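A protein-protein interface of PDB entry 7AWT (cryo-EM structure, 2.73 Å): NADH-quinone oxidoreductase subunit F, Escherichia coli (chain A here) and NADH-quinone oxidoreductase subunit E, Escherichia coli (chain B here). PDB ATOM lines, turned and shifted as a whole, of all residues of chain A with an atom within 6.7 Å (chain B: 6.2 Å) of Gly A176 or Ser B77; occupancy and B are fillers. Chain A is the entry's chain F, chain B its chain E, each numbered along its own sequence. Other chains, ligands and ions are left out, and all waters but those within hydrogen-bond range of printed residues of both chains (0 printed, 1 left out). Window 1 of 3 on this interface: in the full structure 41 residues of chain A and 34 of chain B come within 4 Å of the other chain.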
ATOM      1  N   ASP A  92      14.750  13.552   7.629  1.00  0.00           N
ATOM      2  CA  ASP A  92      13.600  12.792   7.169  1.00  0.00           C
ATOM      3  C   ASP A  92      13.550  11.493   7.948  1.00  0.00           C
ATOM      4  O   ASP A  92      14.321  10.572   7.675  1.00  0.00           O
ATOM      5  CB  ASP A  92      13.691  12.515   5.670  1.00  0.00           C
ATOM      6  CG  ASP A  92      12.587  11.603   5.171  1.00  0.00           C
ATOM      7  OD1 ASP A  92      12.648  10.384   5.427  1.00  0.00           O
ATOM      8  OD2 ASP A  92      11.657  12.105   4.507  1.00  0.00           O
ATOM      9  N   MET A  94      11.269   8.668   8.577  1.00  0.00           N
ATOM     10  CA  MET A  94      10.131   7.815   8.268  1.00  0.00           C
ATOM     11  C   MET A  94      10.578   6.379   8.462  1.00  0.00           C
ATOM     12  O   MET A  94      11.460   5.897   7.746  1.00  0.00           O
ATOM     13  CB  MET A  94       9.628   8.047   6.847  1.00  0.00           C
ATOM     14  CG  MET A  94       9.042   9.417   6.623  1.00  0.00           C
ATOM     15  SD  MET A  94       7.885   9.465   5.252  1.00  0.00           S
ATOM     16  CE  MET A  94       7.521  11.211   5.228  1.00  0.00           C
ATOM     17  N   ARG A 133      11.339  16.380   7.367  1.00  0.00           N
ATOM     18  CA  ARG A 133      10.322  15.385   7.057  1.00  0.00           C
ATOM     19  C   ARG A 133       9.144  15.996   6.315  1.00  0.00           C
ATOM     20  O   ARG A 133       8.711  15.470   5.284  1.00  0.00           O
ATOM     21  CB  ARG A 133       9.857  14.725   8.350  1.00  0.00           C
ATOM     22  CG  ARG A 133       9.021  13.494   8.175  1.00  0.00           C
ATOM     23  CD  ARG A 133       8.539  13.041   9.525  1.00  0.00           C
ATOM     24  NE  ARG A 133       8.251  11.619   9.561  1.00  0.00           N
ATOM     25  CZ  ARG A 133       7.076  11.098   9.250  1.00  0.00           C
ATOM     26  NH1 ARG A 133       6.080  11.886   8.878  1.00  0.00           N
ATOM     27  NH2 ARG A 133       6.895   9.790   9.308  1.00  0.00           N
ATOM     28  N   GLY A 134       8.608  17.098   6.825  1.00  0.00           N
ATOM     29  CA  GLY A 134       7.443  17.712   6.226  1.00  0.00           C
ATOM     30  C   GLY A 134       6.237  17.616   7.133  1.00  0.00           C
ATOM     31  O   GLY A 134       5.465  18.567   7.260  1.00  0.00           O
ATOM     32  N   GLU A 135       6.132  16.544   7.879  1.00  0.00           N
ATOM     33  CA  GLU A 135       5.066  16.362   8.799  1.00  0.00           C
ATOM     34  C   GLU A 135       5.547  16.850  10.137  1.00  0.00           C
ATOM     35  O   GLU A 135       4.836  16.769  11.094  1.00  0.00           O
ATOM     36  CB  GLU A 135       4.701  14.903   8.828  1.00  0.00           C
ATOM     37  CG  GLU A 135       3.804  14.484   7.672  1.00  0.00           C
ATOM     38  CD  GLU A 135       4.400  13.552   6.606  1.00  0.00           C
ATOM     39  OE1 GLU A 135       3.937  12.388   6.490  1.00  0.00           O
ATOM     40  OE2 GLU A 135       5.274  13.982   5.826  1.00  0.00           O
ATOM     41  N   GLY A 174      10.323  18.459   2.914  1.00  0.00           N
ATOM     42  CA  GLY A 174       9.867  17.817   1.705  1.00  0.00           C
ATOM     43  C   GLY A 174       8.513  17.142   1.857  1.00  0.00           C
ATOM     44  O   GLY A 174       7.953  17.034   2.942  1.00  0.00           O
ATOM     45  N   ALA A 175       7.994  16.686   0.722  1.00  0.00           N
ATOM     46  CA  ALA A 175       6.748  15.940   0.699  1.00  0.00           C
ATOM     47  C   ALA A 175       6.975  14.522   1.212  1.00  0.00           C
ATOM     48  O   ALA A 175       8.106  14.037   1.296  1.00  0.00           O
ATOM     49  CB  ALA A 175       6.166  15.911  -0.708  1.00  0.00           C
ATOM     50  N   GLY A 176       5.880  13.853   1.550  1.00  0.00           N
ATOM     51  CA  GLY A 176       5.985  12.635   2.325  1.00  0.00           C
ATOM     52  C   GLY A 176       6.173  11.352   1.546  1.00  0.00           C
ATOM     53  O   GLY A 176       5.204  10.764   1.063  1.00  0.00           O
ATOM     54  N   ARG A 177       7.419  10.898   1.438  1.00  0.00           N
ATOM     55  CA  ARG A 177       7.736   9.587   0.891  1.00  0.00           C
ATOM     56  C   ARG A 177       8.829   8.965   1.743  1.00  0.00           C
ATOM     57  O   ARG A 177       9.842   9.612   2.027  1.00  0.00           O
ATOM     58  CB  ARG A 177       8.182   9.679  -0.567  1.00  0.00           C
ATOM     59  CG  ARG A 177       7.059   9.514  -1.566  1.00  0.00           C
ATOM     60  CD  ARG A 177       6.622   8.071  -1.685  1.00  0.00           C
ATOM     61  NE  ARG A 177       5.660   7.886  -2.766  1.00  0.00           N
ATOM     62  CZ  ARG A 177       4.367   7.646  -2.581  1.00  0.00           C
ATOM     63  NH1 ARG A 177       3.878   7.560  -1.355  1.00  0.00           N
ATOM     64  NH2 ARG A 177       3.564   7.491  -3.622  1.00  0.00           N
ATOM     65  N   TYR A 178       8.624   7.713   2.153  1.00  0.00           N
ATOM     66  CA  TYR A 178       9.560   7.065   3.063  1.00  0.00           C
ATOM     67  C   TYR A 178      10.884   6.748   2.386  1.00  0.00           C
ATOM     68  O   TYR A 178      11.922   6.694   3.053  1.00  0.00           O
ATOM     69  CB  TYR A 178       8.929   5.799   3.635  1.00  0.00           C
ATOM     70  CG  TYR A 178       9.900   4.719   4.037  1.00  0.00           C
ATOM     71  CD1 TYR A 178      10.671   4.848   5.171  1.00  0.00           C
ATOM     72  CD2 TYR A 178      10.024   3.558   3.298  1.00  0.00           C
ATOM     73  CE1 TYR A 178      11.551   3.865   5.550  1.00  0.00           C
ATOM     74  CE2 TYR A 178      10.900   2.570   3.671  1.00  0.00           C
ATOM     75  CZ  TYR A 178      11.661   2.729   4.800  1.00  0.00           C
ATOM     76  OH  TYR A 178      12.541   1.746   5.182  1.00  0.00           O
ATOM     77  N   CYS A 180      12.668   8.558   0.508  1.00  0.00           N
ATOM     78  CA  CYS A 180      13.620   9.662   0.544  1.00  0.00           C
ATOM     79  C   CYS A 180      14.535   9.609   1.757  1.00  0.00           C
ATOM     80  O   CYS A 180      15.495  10.379   1.819  1.00  0.00           O
ATOM     81  CB  CYS A 180      12.892  11.005   0.516  1.00  0.00           C
ATOM     82  SG  CYS A 180      11.388  11.022  -0.459  1.00  0.00           S
ATOM     83  N   GLU A 349       4.929   2.092  -0.214  1.00  0.00           N
ATOM     84  CA  GLU A 349       5.925   3.102   0.067  1.00  0.00           C
ATOM     85  C   GLU A 349       7.178   2.982  -0.617  1.00  0.00           C
ATOM     86  O   GLU A 349       8.102   3.668  -0.351  1.00  0.00           O
ATOM     87  CB  GLU A 349       6.291   3.156   1.485  1.00  0.00           C
ATOM     88  CG  GLU A 349       6.585   4.582   1.731  1.00  0.00           C
ATOM     89  CD  GLU A 349       5.325   5.360   1.783  1.00  0.00           C
ATOM     90  OE1 GLU A 349       5.106   6.285   1.030  1.00  0.00           O
ATOM     91  OE2 GLU A 349       4.495   5.025   2.585  1.00  0.00           O
ATOM     92  N   ALA B  73       5.575  15.781  -8.982  1.00  0.00           N
ATOM     93  CA  ALA B  73       4.307  16.008  -8.299  1.00  0.00           C
ATOM     94  C   ALA B  73       3.532  14.717  -8.086  1.00  0.00           C
ATOM     95  O   ALA B  73       2.842  14.576  -7.071  1.00  0.00           O
ATOM     96  CB  ALA B  73       3.459  17.005  -9.082  1.00  0.00           C
ATOM     97  N   THR B  74       3.619  13.774  -9.021  1.00  0.00           N
ATOM     98  CA  THR B  74       2.896  12.518  -8.901  1.00  0.00           C
ATOM     99  C   THR B  74       3.691  11.434  -8.191  1.00  0.00           C
ATOM    100  O   THR B  74       3.117  10.398  -7.844  1.00  0.00           O
ATOM    101  CB  THR B  74       2.478  12.019 -10.280  1.00  0.00           C
ATOM    102  OG1 THR B  74       3.582  12.146 -11.178  1.00  0.00           O
ATOM    103  CG2 THR B  74       1.327  12.840 -10.803  1.00  0.00           C
ATOM    104  N   PHE B  75       4.990  11.638  -7.971  1.00  0.00           N
ATOM    105  CA  PHE B  75       5.745  10.713  -7.134  1.00  0.00           C
ATOM    106  C   PHE B  75       5.384  10.892  -5.668  1.00  0.00           C
ATOM    107  O   PHE B  75       4.933   9.952  -5.006  1.00  0.00           O
ATOM    108  CB  PHE B  75       7.244  10.916  -7.342  1.00  0.00           C
ATOM    109  CG  PHE B  75       8.096   9.965  -6.555  1.00  0.00           C
ATOM    110  CD1 PHE B  75       8.378   8.706  -7.041  1.00  0.00           C
ATOM    111  CD2 PHE B  75       8.612  10.329  -5.330  1.00  0.00           C
ATOM    112  CE1 PHE B  75       9.154   7.834  -6.322  1.00  0.00           C
ATOM    113  CE2 PHE B  75       9.389   9.457  -4.608  1.00  0.00           C
ATOM    114  CZ  PHE B  75       9.660   8.209  -5.105  1.00  0.00           C
ATOM    115  N   TYR B  76       5.575  12.099  -5.145  1.00  0.00           N
ATOM    116  CA  TYR B  76       5.372  12.347  -3.726  1.00  0.00           C
ATOM    117  C   TYR B  76       3.888  12.364  -3.385  1.00  0.00           C
ATOM    118  O   TYR B  76       3.057  12.805  -4.181  1.00  0.00           O
ATOM    119  CB  TYR B  76       6.023  13.664  -3.330  1.00  0.00           C
ATOM    120  CG  TYR B  76       7.503  13.697  -3.603  1.00  0.00           C
ATOM    121  CD1 TYR B  76       8.391  12.994  -2.808  1.00  0.00           C
ATOM    122  CD2 TYR B  76       8.014  14.421  -4.662  1.00  0.00           C
ATOM    123  CE1 TYR B  76       9.740  13.018  -3.059  1.00  0.00           C
ATOM    124  CE2 TYR B  76       9.362  14.449  -4.920  1.00  0.00           C
ATOM    125  CZ  TYR B  76      10.219  13.749  -4.113  1.00  0.00           C
ATOM    126  OH  TYR B  76      11.566  13.780  -4.372  1.00  0.00           O
ATOM    127  N   SER B  77       3.562  11.882  -2.189  1.00  0.00           N
ATOM    128  CA  SER B  77       2.179  11.662  -1.798  1.00  0.00           C
ATOM    129  C   SER B  77       1.526  12.878  -1.159  1.00  0.00           C
ATOM    130  O   SER B  77       0.300  12.890  -1.013  1.00  0.00           O
ATOM    131  CB  SER B  77       2.089  10.481  -0.832  1.00  0.00           C
ATOM    132  OG  SER B  77       3.021  10.617   0.223  1.00  0.00           O
ATOM    133  N   GLN B  78       2.298  13.890  -0.772  1.00  0.00           N
ATOM    134  CA  GLN B  78       1.748  15.093  -0.167  1.00  0.00           C
ATOM    135  C   GLN B  78       1.738  16.275  -1.127  1.00  0.00           C
ATOM    136  O   GLN B  78       1.590  17.419  -0.690  1.00  0.00           O
ATOM    137  CB  GLN B  78       2.517  15.447   1.102  1.00  0.00           C
ATOM    138  CG  GLN B  78       2.648  14.297   2.077  1.00  0.00           C
ATOM    139  CD  GLN B  78       1.310  13.764   2.534  1.00  0.00           C
ATOM    140  OE1 GLN B  78       0.390  14.528   2.814  1.00  0.00           O
ATOM    141  NE2 GLN B  78       1.196  12.447   2.618  1.00  0.00           N
ATOM    142  N   ILE B  79       1.905  16.021  -2.419  1.00  0.00           N
ATOM    143  CA  ILE B  79       1.681  17.012  -3.462  1.00  0.00           C
ATOM    144  C   ILE B  79       0.419  16.574  -4.191  1.00  0.00           C
ATOM    145  O   ILE B  79       0.474  15.743  -5.104  1.00  0.00           O
ATOM    146  CB  ILE B  79       2.868  17.127  -4.420  1.00  0.00           C
ATOM    147  CG1 ILE B  79       4.145  17.445  -3.651  1.00  0.00           C
ATOM    148  CG2 ILE B  79       2.607  18.201  -5.447  1.00  0.00           C
ATOM    149  CD1 ILE B  79       4.088  18.746  -2.928  1.00  0.00           C
ATOM    150  N   PHE B  80      -0.726  17.112  -3.785  1.00  0.00           N
ATOM    151  CA  PHE B  80      -2.004  16.649  -4.303  1.00  0.00           C
ATOM    152  C   PHE B  80      -2.219  17.158  -5.719  1.00  0.00           C
ATOM    153  O   PHE B  80      -2.064  18.352  -5.989  1.00  0.00           O
ATOM    154  CB  PHE B  80      -3.143  17.109  -3.398  1.00  0.00           C
ATOM    155  CG  PHE B  80      -3.000  16.659  -1.981  1.00  0.00           C
ATOM    156  CD1 PHE B  80      -2.890  15.318  -1.679  1.00  0.00           C
ATOM    157  CD2 PHE B  80      -2.968  17.576  -0.951  1.00  0.00           C
ATOM    158  CE1 PHE B  80      -2.752  14.902  -0.380  1.00  0.00           C
ATOM    159  CE2 PHE B  80      -2.832  17.163   0.350  1.00  0.00           C
ATOM    160  CZ  PHE B  80      -2.725  15.824   0.637  1.00  0.00           C
ATOM    161  N   LEU B 129      -7.556  10.729   4.302  1.00  0.00           N
ATOM    162  CA  LEU B 129      -6.426  10.028   3.718  1.00  0.00           C
ATOM    163  C   LEU B 129      -5.690   9.249   4.795  1.00  0.00           C
ATOM    164  O   LEU B 129      -5.670   9.662   5.958  1.00  0.00           O
ATOM    165  CB  LEU B 129      -5.444  10.998   3.046  1.00  0.00           C
ATOM    166  CG  LEU B 129      -5.920  11.761   1.817  1.00  0.00           C
ATOM    167  CD1 LEU B 129      -4.841  12.710   1.363  1.00  0.00           C
ATOM    168  CD2 LEU B 129      -6.275  10.794   0.713  1.00  0.00           C
ATOM    169  N   CYS B 132       1.674   7.370   6.081  1.00  0.00           N
ATOM    170  CA  CYS B 132       2.633   6.309   6.367  1.00  0.00           C
ATOM    171  C   CYS B 132       2.879   6.167   7.865  1.00  0.00           C
ATOM    172  O   CYS B 132       2.582   5.128   8.462  1.00  0.00           O
ATOM    173  CB  CYS B 132       3.943   6.580   5.625  1.00  0.00           C
ATOM    174  SG  CYS B 132       4.584   8.251   5.806  1.00  0.00           S
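Ala A175 touches Tyr B76. Ile B79 touches Ala A175. Gly A176 touches Gln B78 (N to CG, 3.3 Å). CG of Arg A177 touches CD1 of Tyr B76, at 3.9 Å. CB of Ser B77 touches NH1 of Arg A177, at 3.5 Å. Tyr B76 touches Cys A180. OE2 of Glu A349 touches CB of Cys B132, 3.5 Å away.
The backbone carbonyl oxygen (O) of Phe B75 lies within hydrogen-bond range of the guanidinium group (NE) of Arg A177, 3.1 Å away. The side-chain sulfur (SG) of Cys B132 lies within hydrogen-bond range of the side-chain sulfur (SD) of Met A94, 3.6 Å away. The backbone carbonyl oxygen of Gly A176 lies close to the side-chain hydroxyl of Ser B77 (2.3 Å).
Printed residues of chain B within 4 Å of Met A94: Cys B132 (3.6 Å). Gly A174 touches none of the printed residues of chain B. Gly A176 touches just these residues of chain B: Ser B77 and Gln B78. Of the printed residues of chain A, Phe B75 touches Arg A177. Printed residues of chain A within 4 Å of Tyr B76: Ala A175 (3.5 Å), Arg A177 (3.9 Å) and Cys A180 (3.7 Å). Of chain A, only Gly A176 (2.3 Å) and Arg A177 (3.5 Å) come within 4 Å of Ser B77. Of the printed residues of chain A, Gln B78 touches Gly A176 (3.3 Å). The nearest residue of chain B that does not touch Gly A176 is Tyr B76 (4.9 Å). The nearest residue of chain A that does not touch Ser B77 is Glu A349 (4.9 Å).
Hydrophobic or aromatic side chains of chain B within 4 Å of the printed part of chain A: Phe B75, Tyr B76 and Ile B79. Hydrophobic or aromatic side chains of chain A within 4 Å of the printed part of chain B: Met A94 and Ala A175. Among the printed residues, 10 pairs touch across the chains.
SD of Met A94 lies within hydrogen-bond range of N of Tyr A178 (3.6 Å). The backbone carbonyl oxygen of Arg A177 sits at hydrogen-bond distance from the side-chain sulfur of Cys A180. The guanidinium group of Arg A177 is in salt-bridge range of the side-chain carboxylate of Glu A349, 3.0 Å away.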
